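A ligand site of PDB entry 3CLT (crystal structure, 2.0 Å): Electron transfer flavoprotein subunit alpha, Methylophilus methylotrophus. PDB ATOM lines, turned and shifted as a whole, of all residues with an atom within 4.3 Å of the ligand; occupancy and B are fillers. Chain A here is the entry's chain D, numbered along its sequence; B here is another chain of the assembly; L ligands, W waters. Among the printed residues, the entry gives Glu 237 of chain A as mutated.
OG of Ser 272 sits at hydrogen-bond distance from N of His 275 (3.1 Å).
The backbone carbonyl oxygen (O) of Val 251 sits at hydrogen-bond distance from a ring nitrogen (ND1) of His 275 (3.2 Å).
OD1 of Asn 289 is in hydrogen-bond range of N of Asp 291, 2.9 Å away.
ND2 of Asn 289 lies within hydrogen-bond range of O of Ile 269 (3.1 Å).
N of Gln 253 lies within hydrogen-bond range of O of Gln 274 (2.9 Å).
The backbone NH (N) of Gly 268 lies within hydrogen-bond range of the backbone carbonyl oxygen (O) of Val 288, at 3.1 Å.
The side-chain amide oxygen (OE1) of Gln 121 of chain B sits at hydrogen-bond distance from the side-chain amide nitrogen (NE2) of Gln 274 (3.5 Å).
The side-chain amide oxygen (OE1) of Gln 183 of chain B is in hydrogen-bond range of the indole nitrogen (NE1) of Trp 38 of chain B (3.0 Å).
Water W7 bridges O5 of the ligand and OD2 of Asp 291.
Water W3 bridges an oxygen (O9) of the ligand (2.5 Å) and the side-chain amide oxygen (OE1) of Gln 274 (2.9 Å).
Water W4 bridges the side-chain hydroxyl (OG1) of Thr 290 and an oxygen (O6) of the ligand.
Water W6 lies within hydrogen-bond range of an oxygen (O13) of the ligand (2.7 Å), the backbone NH of Ser 272 (2.9 Å) and the backbone NH of Gly 271 (3.1 Å).
The side-chain hydroxyl of Ser 236 lies within hydrogen-bond range of an oxygen (O14) of the ligand.
N of Ser 270 lies within hydrogen-bond range of O13 of the ligand, at 2.8 Å.
An oxygen (O2) of the ligand lies within hydrogen-bond range of the side-chain hydroxyl (OG) of Ser 270 (2.7 Å).
The side-chain hydroxyl (OG) of Ser 272 is in hydrogen-bond range of an oxygen (O11) of the ligand (2.7 Å).
The backbone carbonyl oxygen of Val 251 sits at hydrogen-bond distance from a nitrogen (N7) of the ligand, at 2.7 Å.
O6 of the ligand lies within hydrogen-bond range of OD1 of Asn 289 (2.8 Å).
ND1 of His 275 sits at hydrogen-bond distance from O7 of the ligand, at 2.8 Å.
N of Arg 211 sits at hydrogen-bond distance from O14 of the ligand (2.9 Å).
NE of Arg 211 lies within salt-bridge range of O1 of the ligand (2.9 Å).
OD2 of Asp 307 sits at hydrogen-bond distance from N3 of the ligand.
O7 of the ligand is in hydrogen-bond range of N of Glu 237 (2.9 Å).
O8 of the ligand is in hydrogen-bond range of NE2 of Gln 250.
The backbone NH (N) of Gly 255 sits at hydrogen-bond distance from an oxygen (O8) of the ligand.
O8 of the ligand sits at hydrogen-bond distance from N of Ser 254, 3.1 Å away.
A nitrogen (N4) of the ligand sits at hydrogen-bond distance from the backbone NH (N) of Ile 308, 3.2 Å away.
An oxygen (O8) of the ligand is in hydrogen-bond range of the backbone NH (N) of Gln 253.
A nitrogen (N5) of the ligand sits at hydrogen-bond distance from the backbone NH (N) of Thr 290 (3.3 Å).
A nitrogen (N5) of the ligand lies close to the side-chain hydroxyl of Thr 290, 3.4 Å away.
OE1 of Gln 274 is in hydrogen-bond range of O9 of the ligand, 3.4 Å away.
O4 of the ligand lies close to O of Gly 268 (3.2 Å).
Merely in contact with the ligand: Gly 210 (3.3 Å), Gly 212 (3.4 Å), Pro 238 (3.4 Å), Gly 252 (3.1 Å), Ile 269 (3.5 Å), Asp 291 (3.2 Å), Ala 306 (3.6 Å), Phe 309 (3.6 Å), Trp 38 of chain B (3.7 Å), Val 120 of chain B (3.9 Å), Gln 121 of chain B (3.7 Å), Gln 183 of chain B (3.4 Å) and Leu 184 of chain B (3.6 Å).
Hydrophobic or aromatic side chains within 4 Å of the ligand: Pro 238, Ile 269, His 275, Ile 308, Phe 309, Trp 38 of chain B, Val 120 of chain B and Leu 184 of chain B.
The nearest printed residue that does not touch the ligand is Val 145 of chain B (4.2 Å).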
ATOM      1  N   GLY A 210      13.102   4.466  16.582  1.00  0.00           N
ATOM      2  CA  GLY A 210      13.555   4.772  17.925  1.00  0.00           C
ATOM      3  C   GLY A 210      14.758   3.948  18.341  1.00  0.00           C
ATOM      4  O   GLY A 210      15.401   3.311  17.512  1.00  0.00           O
ATOM      5  N   ARG A 211      15.041   3.961  19.635  1.00  0.00           N
ATOM      6  CA  ARG A 211      16.246   3.340  20.175  1.00  0.00           C
ATOM      7  C   ARG A 211      16.321   1.845  19.867  1.00  0.00           C
ATOM      8  O   ARG A 211      17.397   1.272  19.875  1.00  0.00           O
ATOM      9  CB  ARG A 211      16.367   3.570  21.707  1.00  0.00           C
ATOM     10  CG  ARG A 211      17.793   3.409  22.213  1.00  0.00           C
ATOM     11  CD  ARG A 211      17.956   3.307  23.741  1.00  0.00           C
ATOM     12  NE  ARG A 211      17.009   4.094  24.528  1.00  0.00           N
ATOM     13  CZ  ARG A 211      17.283   5.230  25.180  1.00  0.00           C
ATOM     14  NH1 ARG A 211      18.473   5.798  25.103  1.00  0.00           N
ATOM     15  NH2 ARG A 211      16.343   5.816  25.892  1.00  0.00           N
ATOM     16  N   GLY A 212      15.179   1.224  19.601  1.00  0.00           N
ATOM     17  CA  GLY A 212      15.121  -0.188  19.269  1.00  0.00           C
ATOM     18  C   GLY A 212      15.856  -0.607  18.016  1.00  0.00           C
ATOM     19  O   GLY A 212      16.070  -1.799  17.820  1.00  0.00           O
ATOM     20  N   SER A 236      12.678   9.296  17.205  1.00  0.00           N
ATOM     21  CA  SER A 236      12.559   9.707  18.583  1.00  0.00           C
ATOM     22  C   SER A 236      13.851  10.406  18.972  1.00  0.00           C
ATOM     23  O   SER A 236      14.816  10.441  18.210  1.00  0.00           O
ATOM     24  CB  SER A 236      12.337   8.475  19.476  1.00  0.00           C
ATOM     25  OG  SER A 236      13.433   7.588  19.359  1.00  0.00           O
ATOM     26  N   GLU A 237      13.889  10.945  20.188  1.00  0.00           N
ATOM     27  CA  GLU A 237      15.017  11.755  20.643  1.00  0.00           C
ATOM     28  C   GLU A 237      16.380  11.041  20.628  1.00  0.00           C
ATOM     29  O   GLU A 237      17.351  11.629  20.187  1.00  0.00           O
ATOM     30  CB  GLU A 237      14.758  12.371  22.027  1.00  0.00           C
ATOM     31  CG  GLU A 237      15.954  13.127  22.530  1.00  0.00           C
ATOM     32  CD  GLU A 237      15.737  13.904  23.801  1.00  0.00           C
ATOM     33  OE1 GLU A 237      14.584  14.102  24.211  1.00  0.00           O
ATOM     34  OE2 GLU A 237      16.739  14.346  24.396  1.00  0.00           O
ATOM     35  N   PRO A 238      16.462   9.785  21.123  1.00  0.00           N
ATOM     36  CA  PRO A 238      17.820   9.174  21.174  1.00  0.00           C
ATOM     37  C   PRO A 238      18.534   9.075  19.812  1.00  0.00           C
ATOM     38  O   PRO A 238      19.783   9.114  19.764  1.00  0.00           O
ATOM     39  CB  PRO A 238      17.578   7.773  21.762  1.00  0.00           C
ATOM     40  CG  PRO A 238      16.162   7.748  22.271  1.00  0.00           C
ATOM     41  CD  PRO A 238      15.413   8.905  21.660  1.00  0.00           C
ATOM     42  N   GLN A 250      13.173  14.892  14.358  1.00  0.00           N
ATOM     43  CA  GLN A 250      12.780  14.438  15.703  1.00  0.00           C
ATOM     44  C   GLN A 250      11.336  14.822  16.014  1.00  0.00           C
ATOM     45  O   GLN A 250      10.963  16.009  15.906  1.00  0.00           O
ATOM     46  CB  GLN A 250      13.692  15.034  16.775  1.00  0.00           C
ATOM     47  CG  GLN A 250      13.338  14.629  18.218  1.00  0.00           C
ATOM     48  CD  GLN A 250      14.339  15.159  19.226  1.00  0.00           C
ATOM     49  OE1 GLN A 250      15.544  15.139  18.980  1.00  0.00           O
ATOM     50  NE2 GLN A 250      13.853  15.633  20.367  1.00  0.00           N
ATOM     51  N   VAL A 251      10.547  13.829  16.439  1.00  0.00           N
ATOM     52  CA  VAL A 251       9.133  14.011  16.796  1.00  0.00           C
ATOM     53  C   VAL A 251       8.989  14.025  18.313  1.00  0.00           C
ATOM     54  O   VAL A 251       9.517  13.144  19.008  1.00  0.00           O
ATOM     55  CB  VAL A 251       8.277  12.844  16.228  1.00  0.00           C
ATOM     56  CG1 VAL A 251       6.816  12.968  16.657  1.00  0.00           C
ATOM     57  CG2 VAL A 251       8.383  12.798  14.705  1.00  0.00           C
ATOM     58  N   GLY A 252       8.270  15.017  18.831  1.00  0.00           N
ATOM     59  CA  GLY A 252       7.967  15.118  20.259  1.00  0.00           C
ATOM     60  C   GLY A 252       8.138  16.516  20.809  1.00  0.00           C
ATOM     61  O   GLY A 252       8.341  17.471  20.049  1.00  0.00           O
ATOM     62  N   GLN A 253       8.085  16.631  22.133  1.00  0.00           N
ATOM     63  CA  GLN A 253       8.102  17.935  22.815  1.00  0.00           C
ATOM     64  C   GLN A 253       9.277  18.836  22.410  1.00  0.00           C
ATOM     65  O   GLN A 253       9.078  19.995  22.042  1.00  0.00           O
ATOM     66  CB  GLN A 253       8.137  17.735  24.328  1.00  0.00           C
ATOM     67  CG  GLN A 253       8.318  19.038  25.096  1.00  0.00           C
ATOM     68  CD  GLN A 253       8.220  18.863  26.595  1.00  0.00           C
ATOM     69  OE1 GLN A 253       7.256  18.301  27.106  1.00  0.00           O
ATOM     70  NE2 GLN A 253       9.220  19.363  27.314  1.00  0.00           N
ATOM     71  N   SER A 254      10.486  18.330  22.542  1.00  0.00           N
ATOM     72  CA  SER A 254      11.698  19.040  22.176  1.00  0.00           C
ATOM     73  C   SER A 254      11.887  19.145  20.648  1.00  0.00           C
ATOM     74  O   SER A 254      12.601  20.012  20.162  1.00  0.00           O
ATOM     75  CB  SER A 254      12.924  18.346  22.799  1.00  0.00           C
ATOM     76  OG  SER A 254      13.109  18.761  24.147  1.00  0.00           O
ATOM     77  N   GLY A 255      11.256  18.223  19.922  1.00  0.00           N
ATOM     78  CA  GLY A 255      11.289  18.236  18.463  1.00  0.00           C
ATOM     79  C   GLY A 255      10.019  18.884  17.933  1.00  0.00           C
ATOM     80  O   GLY A 255       9.567  19.903  18.468  1.00  0.00           O
ATOM     81  N   GLY A 268      10.297   0.523  17.092  1.00  0.00           N
ATOM     82  CA  GLY A 268      11.321   0.543  18.133  1.00  0.00           C
ATOM     83  C   GLY A 268      11.248   1.797  19.006  1.00  0.00           C
ATOM     84  O   GLY A 268      12.287   2.277  19.465  1.00  0.00           O
ATOM     85  N   ILE A 269      10.044   2.307  19.221  1.00  0.00           N
ATOM     86  CA  ILE A 269       9.777   3.495  20.039  1.00  0.00           C
ATOM     87  C   ILE A 269       8.823   3.113  21.201  1.00  0.00           C
ATOM     88  O   ILE A 269       7.705   2.624  20.958  1.00  0.00           O
ATOM     89  CB  ILE A 269       9.131   4.624  19.186  1.00  0.00           C
ATOM     90  CG1 ILE A 269      10.126   5.184  18.166  1.00  0.00           C
ATOM     91  CG2 ILE A 269       8.650   5.776  20.089  1.00  0.00           C
ATOM     92  CD1 ILE A 269       9.495   5.916  17.007  1.00  0.00           C
ATOM     93  N   SER A 270       9.252   3.346  22.448  1.00  0.00           N
ATOM     94  CA  SER A 270       8.444   2.938  23.617  1.00  0.00           C
ATOM     95  C   SER A 270       7.151   3.724  23.801  1.00  0.00           C
ATOM     96  O   SER A 270       6.182   3.206  24.374  1.00  0.00           O
ATOM     97  CB  SER A 270       9.270   3.005  24.916  1.00  0.00           C
ATOM     98  OG  SER A 270       9.651   4.335  25.251  1.00  0.00           O
ATOM     99  N   GLY A 271       7.128   4.960  23.330  1.00  0.00           N
ATOM    100  CA  GLY A 271       5.997   5.865  23.530  1.00  0.00           C
ATOM    101  C   GLY A 271       6.068   6.672  24.813  1.00  0.00           C
ATOM    102  O   GLY A 271       5.069   6.786  25.517  1.00  0.00           O
ATOM    103  N   SER A 272       7.223   7.253  25.110  1.00  0.00           N
ATOM    104  CA  SER A 272       7.335   8.205  26.217  1.00  0.00           C
ATOM    105  C   SER A 272       6.316   9.334  26.028  1.00  0.00           C
ATOM    106  O   SER A 272       5.895   9.634  24.926  1.00  0.00           O
ATOM    107  CB  SER A 272       8.726   8.808  26.274  1.00  0.00           C
ATOM    108  OG  SER A 272       8.905   9.733  25.210  1.00  0.00           O
ATOM    109  N   GLN A 274       6.793  12.498  26.209  1.00  0.00           N
ATOM    110  CA  GLN A 274       7.358  13.537  25.347  1.00  0.00           C
ATOM    111  C   GLN A 274       7.346  13.170  23.861  1.00  0.00           C
ATOM    112  O   GLN A 274       7.185  14.050  23.012  1.00  0.00           O
ATOM    113  CB  GLN A 274       8.763  13.920  25.819  1.00  0.00           C
ATOM    114  CG  GLN A 274       8.814  14.531  27.216  1.00  0.00           C
ATOM    115  CD  GLN A 274       8.905  13.493  28.339  1.00  0.00           C
ATOM    116  OE1 GLN A 274       8.757  12.277  28.143  1.00  0.00           O
ATOM    117  NE2 GLN A 274       9.146  13.991  29.551  1.00  0.00           N
ATOM    118  N   HIS A 275       7.487  11.890  23.525  1.00  0.00           N
ATOM    119  CA  HIS A 275       7.313  11.478  22.134  1.00  0.00           C
ATOM    120  C   HIS A 275       5.845  11.592  21.692  1.00  0.00           C
ATOM    121  O   HIS A 275       5.543  12.117  20.613  1.00  0.00           O
ATOM    122  CB  HIS A 275       7.841  10.068  21.869  1.00  0.00           C
ATOM    123  CG  HIS A 275       7.969   9.757  20.416  1.00  0.00           C
ATOM    124  ND1 HIS A 275       9.092  10.068  19.683  1.00  0.00           N
ATOM    125  CD2 HIS A 275       7.073   9.227  19.532  1.00  0.00           C
ATOM    126  CE1 HIS A 275       8.895   9.728  18.422  1.00  0.00           C
ATOM    127  NE2 HIS A 275       7.684   9.215  18.297  1.00  0.00           N
ATOM    128  N   VAL A 288       5.247  -0.958  16.074  1.00  0.00           N
ATOM    129  CA  VAL A 288       5.987  -2.219  15.931  1.00  0.00           C
ATOM    130  C   VAL A 288       7.058  -2.257  17.026  1.00  0.00           C
ATOM    131  O   VAL A 288       8.023  -1.517  16.996  1.00  0.00           O
ATOM    132  CB  VAL A 288       6.658  -2.362  14.556  1.00  0.00           C
ATOM    133  CG1 VAL A 288       7.133  -3.801  14.347  1.00  0.00           C
ATOM    134  CG2 VAL A 288       5.705  -1.927  13.440  1.00  0.00           C
ATOM    135  N   ASN A 289       6.857  -3.145  17.995  1.00  0.00           N
ATOM    136  CA  ASN A 289       7.634  -3.130  19.224  1.00  0.00           C
ATOM    137  C   ASN A 289       7.520  -4.493  19.915  1.00  0.00           C
ATOM    138  O   ASN A 289       6.410  -5.003  20.092  1.00  0.00           O
ATOM    139  CB  ASN A 289       7.097  -2.020  20.134  1.00  0.00           C
ATOM    140  CG  ASN A 289       8.053  -1.667  21.269  1.00  0.00           C
ATOM    141  OD1 ASN A 289       8.582  -2.548  21.936  1.00  0.00           O
ATOM    142  ND2 ASN A 289       8.241  -0.365  21.498  1.00  0.00           N
ATOM    143  N   THR A 290       8.648  -5.082  20.288  1.00  0.00           N
ATOM    144  CA  THR A 290       8.671  -6.398  20.912  1.00  0.00           C
ATOM    145  C   THR A 290       8.270  -6.387  22.411  1.00  0.00           C
ATOM    146  O   THR A 290       8.149  -7.434  23.037  1.00  0.00           O
ATOM    147  CB  THR A 290      10.069  -7.050  20.767  1.00  0.00           C
ATOM    148  OG1 THR A 290      11.078  -6.104  21.126  1.00  0.00           O
ATOM    149  CG2 THR A 290      10.293  -7.533  19.340  1.00  0.00           C
ATOM    150  N   ASP A 291       8.060  -5.191  22.983  1.00  0.00           N
ATOM    151  CA  ASP A 291       7.599  -5.083  24.368  1.00  0.00           C
ATOM    152  C   ASP A 291       6.095  -4.807  24.398  1.00  0.00           C
ATOM    153  O   ASP A 291       5.671  -3.668  24.185  1.00  0.00           O
ATOM    154  CB  ASP A 291       8.341  -3.943  25.089  1.00  0.00           C
ATOM    155  CG  ASP A 291       7.900  -3.792  26.551  1.00  0.00           C
ATOM    156  OD1 ASP A 291       7.171  -4.675  27.059  1.00  0.00           O
ATOM    157  OD2 ASP A 291       8.311  -2.781  27.179  1.00  0.00           O
ATOM    158  N   ALA A 294       4.918  -1.723  26.250  1.00  0.00           N
ATOM    159  CA  ALA A 294       5.338  -0.384  25.814  1.00  0.00           C
ATOM    160  C   ALA A 294       4.152   0.594  25.774  1.00  0.00           C
ATOM    161  O   ALA A 294       3.073   0.254  25.278  1.00  0.00           O
ATOM    162  CB  ALA A 294       6.033  -0.452  24.457  1.00  0.00           C
ATOM    163  N   ALA A 306       6.517  -7.618  17.337  1.00  0.00           N
ATOM    164  CA  ALA A 306       7.489  -8.350  16.527  1.00  0.00           C
ATOM    165  C   ALA A 306       8.753  -7.538  16.308  1.00  0.00           C
ATOM    166  O   ALA A 306       8.755  -6.314  16.483  1.00  0.00           O
ATOM    167  CB  ALA A 306       6.876  -8.721  15.194  1.00  0.00           C
ATOM    168  N   ASP A 307       9.815  -8.232  15.924  1.00  0.00           N
ATOM    169  CA  ASP A 307      11.113  -7.645  15.653  1.00  0.00           C
ATOM    170  C   ASP A 307      11.042  -6.693  14.457  1.00  0.00           C
ATOM    171  O   ASP A 307      10.572  -7.072  13.400  1.00  0.00           O
ATOM    172  CB  ASP A 307      12.130  -8.760  15.373  1.00  0.00           C
ATOM    173  CG  ASP A 307      13.518  -8.223  15.129  1.00  0.00           C
ATOM    174  OD1 ASP A 307      13.924  -8.133  13.945  1.00  0.00           O
ATOM    175  OD2 ASP A 307      14.203  -7.867  16.112  1.00  0.00           O
ATOM    176  N   ILE A 308      11.501  -5.467  14.651  1.00  0.00           N
ATOM    177  CA  ILE A 308      11.394  -4.424  13.633  1.00  0.00           C
ATOM    178  C   ILE A 308      12.226  -4.715  12.393  1.00  0.00           C
ATOM    179  O   ILE A 308      11.865  -4.303  11.295  1.00  0.00           O
ATOM    180  CB  ILE A 308      11.734  -2.995  14.182  1.00  0.00           C
ATOM    181  CG1 ILE A 308      13.141  -2.940  14.833  1.00  0.00           C
ATOM    182  CG2 ILE A 308      10.646  -2.534  15.134  1.00  0.00           C
ATOM    183  CD1 ILE A 308      13.545  -1.554  15.294  1.00  0.00           C
ATOM    184  N   PHE A 309      13.332  -5.434  12.544  1.00  0.00           N
ATOM    185  CA  PHE A 309      14.205  -5.735  11.397  1.00  0.00           C
ATOM    186  C   PHE A 309      13.553  -6.790  10.514  1.00  0.00           C
ATOM    187  O   PHE A 309      13.526  -6.647   9.287  1.00  0.00           O
ATOM    188  CB  PHE A 309      15.600  -6.168  11.859  1.00  0.00           C
ATOM    189  CG  PHE A 309      16.185  -5.275  12.932  1.00  0.00           C
ATOM    190  CD1 PHE A 309      16.208  -5.697  14.257  1.00  0.00           C
ATOM    191  CD2 PHE A 309      16.697  -4.028  12.624  1.00  0.00           C
ATOM    192  CE1 PHE A 309      16.742  -4.890  15.261  1.00  0.00           C
ATOM    193  CE2 PHE A 309      17.225  -3.211  13.599  1.00  0.00           C
ATOM    194  CZ  PHE A 309      17.260  -3.633  14.932  1.00  0.00           C
ATOM    195  N   TRP B  38      19.048   9.982  32.983  1.00  0.00           N
ATOM    196  CA  TRP B  38      19.532  11.379  33.029  1.00  0.00           C
ATOM    197  C   TRP B  38      20.837  11.539  33.806  1.00  0.00           C
ATOM    198  O   TRP B  38      21.678  12.389  33.474  1.00  0.00           O
ATOM    199  CB  TRP B  38      18.438  12.310  33.605  1.00  0.00           C
ATOM    200  CG  TRP B  38      17.395  12.663  32.588  1.00  0.00           C
ATOM    201  CD1 TRP B  38      17.347  13.795  31.823  1.00  0.00           C
ATOM    202  CD2 TRP B  38      16.269  11.867  32.196  1.00  0.00           C
ATOM    203  NE1 TRP B  38      16.248  13.759  30.993  1.00  0.00           N
ATOM    204  CE2 TRP B  38      15.574  12.587  31.191  1.00  0.00           C
ATOM    205  CE3 TRP B  38      15.754  10.625  32.603  1.00  0.00           C
ATOM    206  CZ2 TRP B  38      14.423  12.101  30.578  1.00  0.00           C
ATOM    207  CZ3 TRP B  38      14.611  10.145  31.990  1.00  0.00           C
ATOM    208  CH2 TRP B  38      13.965  10.879  30.985  1.00  0.00           C
ATOM    209  N   VAL B 120      17.180  16.145  34.659  1.00  0.00           N
ATOM    210  CA  VAL B 120      15.910  16.845  34.395  1.00  0.00           C
ATOM    211  C   VAL B 120      14.747  16.184  35.122  1.00  0.00           C
ATOM    212  O   VAL B 120      13.952  16.879  35.757  1.00  0.00           O
ATOM    213  CB  VAL B 120      15.607  16.945  32.876  1.00  0.00           C
ATOM    214  CG1 VAL B 120      14.141  17.299  32.613  1.00  0.00           C
ATOM    215  CG2 VAL B 120      16.514  17.980  32.241  1.00  0.00           C
ATOM    216  N   GLN B 121      14.655  14.858  35.005  1.00  0.00           N
ATOM    217  CA  GLN B 121      13.630  14.070  35.680  1.00  0.00           C
ATOM    218  C   GLN B 121      14.090  12.627  35.888  1.00  0.00           C
ATOM    219  O   GLN B 121      15.129  12.218  35.370  1.00  0.00           O
ATOM    220  CB  GLN B 121      12.328  14.094  34.880  1.00  0.00           C
ATOM    221  CG  GLN B 121      12.438  13.452  33.505  1.00  0.00           C
ATOM    222  CD  GLN B 121      11.129  13.450  32.756  1.00  0.00           C
ATOM    223  OE1 GLN B 121      10.691  12.423  32.249  1.00  0.00           O
ATOM    224  NE2 GLN B 121      10.469  14.605  32.716  1.00  0.00           N
ATOM    225  N   VAL B 145      16.714  21.893  32.367  1.00  0.00           N
ATOM    226  CA  VAL B 145      16.721  21.322  31.013  1.00  0.00           C
ATOM    227  C   VAL B 145      17.912  21.828  30.209  1.00  0.00           C
ATOM    228  O   VAL B 145      17.766  22.348  29.094  1.00  0.00           O
ATOM    229  CB  VAL B 145      15.371  21.479  30.269  1.00  0.00           C
ATOM    230  CG1 VAL B 145      15.270  20.472  29.129  1.00  0.00           C
ATOM    231  CG2 VAL B 145      14.181  21.310  31.233  1.00  0.00           C
ATOM    232  N   GLN B 183      19.844  17.658  30.673  1.00  0.00           N
ATOM    233  CA  GLN B 183      19.014  16.946  29.716  1.00  0.00           C
ATOM    234  C   GLN B 183      19.799  15.891  28.935  1.00  0.00           C
ATOM    235  O   GLN B 183      20.998  16.033  28.666  1.00  0.00           O
ATOM    236  CB  GLN B 183      18.379  17.966  28.762  1.00  0.00           C
ATOM    237  CG  GLN B 183      17.665  17.415  27.540  1.00  0.00           C
ATOM    238  CD  GLN B 183      16.417  16.594  27.839  1.00  0.00           C
ATOM    239  OE1 GLN B 183      16.291  15.943  28.899  1.00  0.00           O
ATOM    240  NE2 GLN B 183      15.500  16.570  26.881  1.00  0.00           N
ATOM    241  N   LEU B 184      19.076  14.845  28.544  1.00  0.00           N
ATOM    242  CA  LEU B 184      19.577  13.852  27.592  1.00  0.00           C
ATOM    243  C   LEU B 184      20.207  14.529  26.374  1.00  0.00           C
ATOM    244  O   LEU B 184      19.718  15.550  25.901  1.00  0.00           O
ATOM    245  CB  LEU B 184      18.419  12.978  27.089  1.00  0.00           C
ATOM    246  CG  LEU B 184      17.538  12.273  28.135  1.00  0.00           C
ATOM    247  CD1 LEU B 184      16.432  11.509  27.438  1.00  0.00           C
ATOM    248  CD2 LEU B 184      18.354  11.343  29.007  1.00  0.00           C
HETATM  249  P1  LIG L   1      13.199   3.629  24.455  1.00  0.00           P
HETATM  250  O1  LIG L   1      14.425   2.992  25.040  1.00  0.00           O
HETATM  251  O2  LIG L   1      12.298   4.166  25.526  1.00  0.00           O
HETATM  252  O3  LIG L   1      12.376   2.546  23.601  1.00  0.00           O
HETATM  253  C1  LIG L   1      13.024   1.596  22.788  1.00  0.00           C
HETATM  254  C2  LIG L   1      11.962   0.605  22.380  1.00  0.00           C
HETATM  255  O4  LIG L   1      12.418  -0.278  21.385  1.00  0.00           O
HETATM  256  C3  LIG L   1      11.499  -0.264  23.550  1.00  0.00           C
HETATM  257  O5  LIG L   1      10.117  -0.074  23.766  1.00  0.00           O
HETATM  258  C4  LIG L   1      11.837  -1.687  23.136  1.00  0.00           C
HETATM  259  O6  LIG L   1      10.861  -2.606  23.543  1.00  0.00           O
HETATM  260  C5  LIG L   1      11.919  -1.563  21.631  1.00  0.00           C
HETATM  261  N1  LIG L   1      12.785  -2.543  20.949  1.00  0.00           N
HETATM  262  C6  LIG L   1      14.089  -2.863  21.231  1.00  0.00           C
HETATM  263  N2  LIG L   1      14.493  -3.779  20.328  1.00  0.00           N
HETATM  264  C7  LIG L   1      13.490  -4.025  19.469  1.00  0.00           C
HETATM  265  C8  LIG L   1      13.367  -4.883  18.371  1.00  0.00           C
HETATM  266  N3  LIG L   1      14.416  -5.575  17.903  1.00  0.00           N
HETATM  267  N4  LIG L   1      12.167  -4.911  17.699  1.00  0.00           N
HETATM  268  C9  LIG L   1      11.101  -4.135  18.092  1.00  0.00           C
HETATM  269  N5  LIG L   1      11.219  -3.305  19.184  1.00  0.00           N
HETATM  270  C10 LIG L   1      12.404  -3.253  19.855  1.00  0.00           C
HETATM  271  N6  LIG L   1      11.541  12.063  23.253  1.00  0.00           N
HETATM  272  C11 LIG L   1      11.221  12.092  21.928  1.00  0.00           C
HETATM  273  O7  LIG L   1      11.195  11.030  21.326  1.00  0.00           O
HETATM  274  N7  LIG L   1      11.007  13.280  21.295  1.00  0.00           N
HETATM  275  C12 LIG L   1      11.085  14.466  22.007  1.00  0.00           C
HETATM  276  O8  LIG L   1      10.978  15.520  21.371  1.00  0.00           O
HETATM  277  C13 LIG L   1      11.403  14.439  23.375  1.00  0.00           C
HETATM  278  N8  LIG L   1      11.485  15.598  24.145  1.00  0.00           N
HETATM  279  C14 LIG L   1      11.809  15.507  25.488  1.00  0.00           C
HETATM  280  C15 LIG L   1      11.887  16.671  26.250  1.00  0.00           C
HETATM  281  C16 LIG L   1      12.199  16.598  27.613  1.00  0.00           C
HETATM  282  C17 LIG L   1      12.108  17.863  28.435  1.00  0.00           C
HETATM  283  C18 LIG L   1      12.440  15.349  28.214  1.00  0.00           C
HETATM  284  C19 LIG L   1      12.583  15.223  29.707  1.00  0.00           C
HETATM  285  C20 LIG L   1      12.354  14.196  27.451  1.00  0.00           C
HETATM  286  C21 LIG L   1      12.050  14.257  26.089  1.00  0.00           C
HETATM  287  N9  LIG L   1      11.980  13.098  25.327  1.00  0.00           N
HETATM  288  C22 LIG L   1      11.632  13.209  23.996  1.00  0.00           C
HETATM  289  C23 LIG L   1      12.815  11.902  25.709  1.00  0.00           C
HETATM  290  C24 LIG L   1      11.954  10.793  26.307  1.00  0.00           C
HETATM  291  O9  LIG L   1      11.824  10.957  27.704  1.00  0.00           O
HETATM  292  C25 LIG L   1      12.495   9.382  26.036  1.00  0.00           C
HETATM  293  O10 LIG L   1      13.823   9.247  26.459  1.00  0.00           O
HETATM  294  C26 LIG L   1      12.467   8.964  24.560  1.00  0.00           C
HETATM  295  O11 LIG L   1      11.243   9.351  23.959  1.00  0.00           O
HETATM  296  C27 LIG L   1      12.696   7.463  24.442  1.00  0.00           C
HETATM  297  O12 LIG L   1      12.924   7.162  23.085  1.00  0.00           O
HETATM  298  P2  LIG L   1      12.691   5.673  22.508  1.00  0.00           P
HETATM  299  O13 LIG L   1      11.245   5.307  22.614  1.00  0.00           O
HETATM  300  O14 LIG L   1      13.204   5.653  21.085  1.00  0.00           O
HETATM  301  O15 LIG L   1      13.667   4.734  23.380  1.00  0.00           O
HETATM  302  O   HOH W   1      16.985  -5.997  19.143  1.00  0.00           O
HETATM  303  O   HOH W   2      13.534  -7.336  20.805  1.00  0.00           O
HETATM  304  O   HOH W   3      10.152   9.960  29.304  1.00  0.00           O
HETATM  305  O   HOH W   4      11.535  -5.201  23.518  1.00  0.00           O
HETATM  306  O   HOH W   5      14.079   7.774  28.552  1.00  0.00           O
HETATM  307  O   HOH W   6       9.359   7.152  23.149  1.00  0.00           O
HETATM  308  O   HOH W   7       9.600  -0.706  26.113  1.00  0.00           O
HETATM  309  O   HOH W   8      15.263   0.611  25.741  1.00  0.00           O
HETATM  310  O   HOH W   9      15.812  -5.879  21.355  1.00  0.00           O
HETATM  311  O   HOH W  10      16.048  10.022  24.666  1.00  0.00           O
HETATM  312  O   HOH W  11      11.666   2.861  28.098  1.00  0.00           O
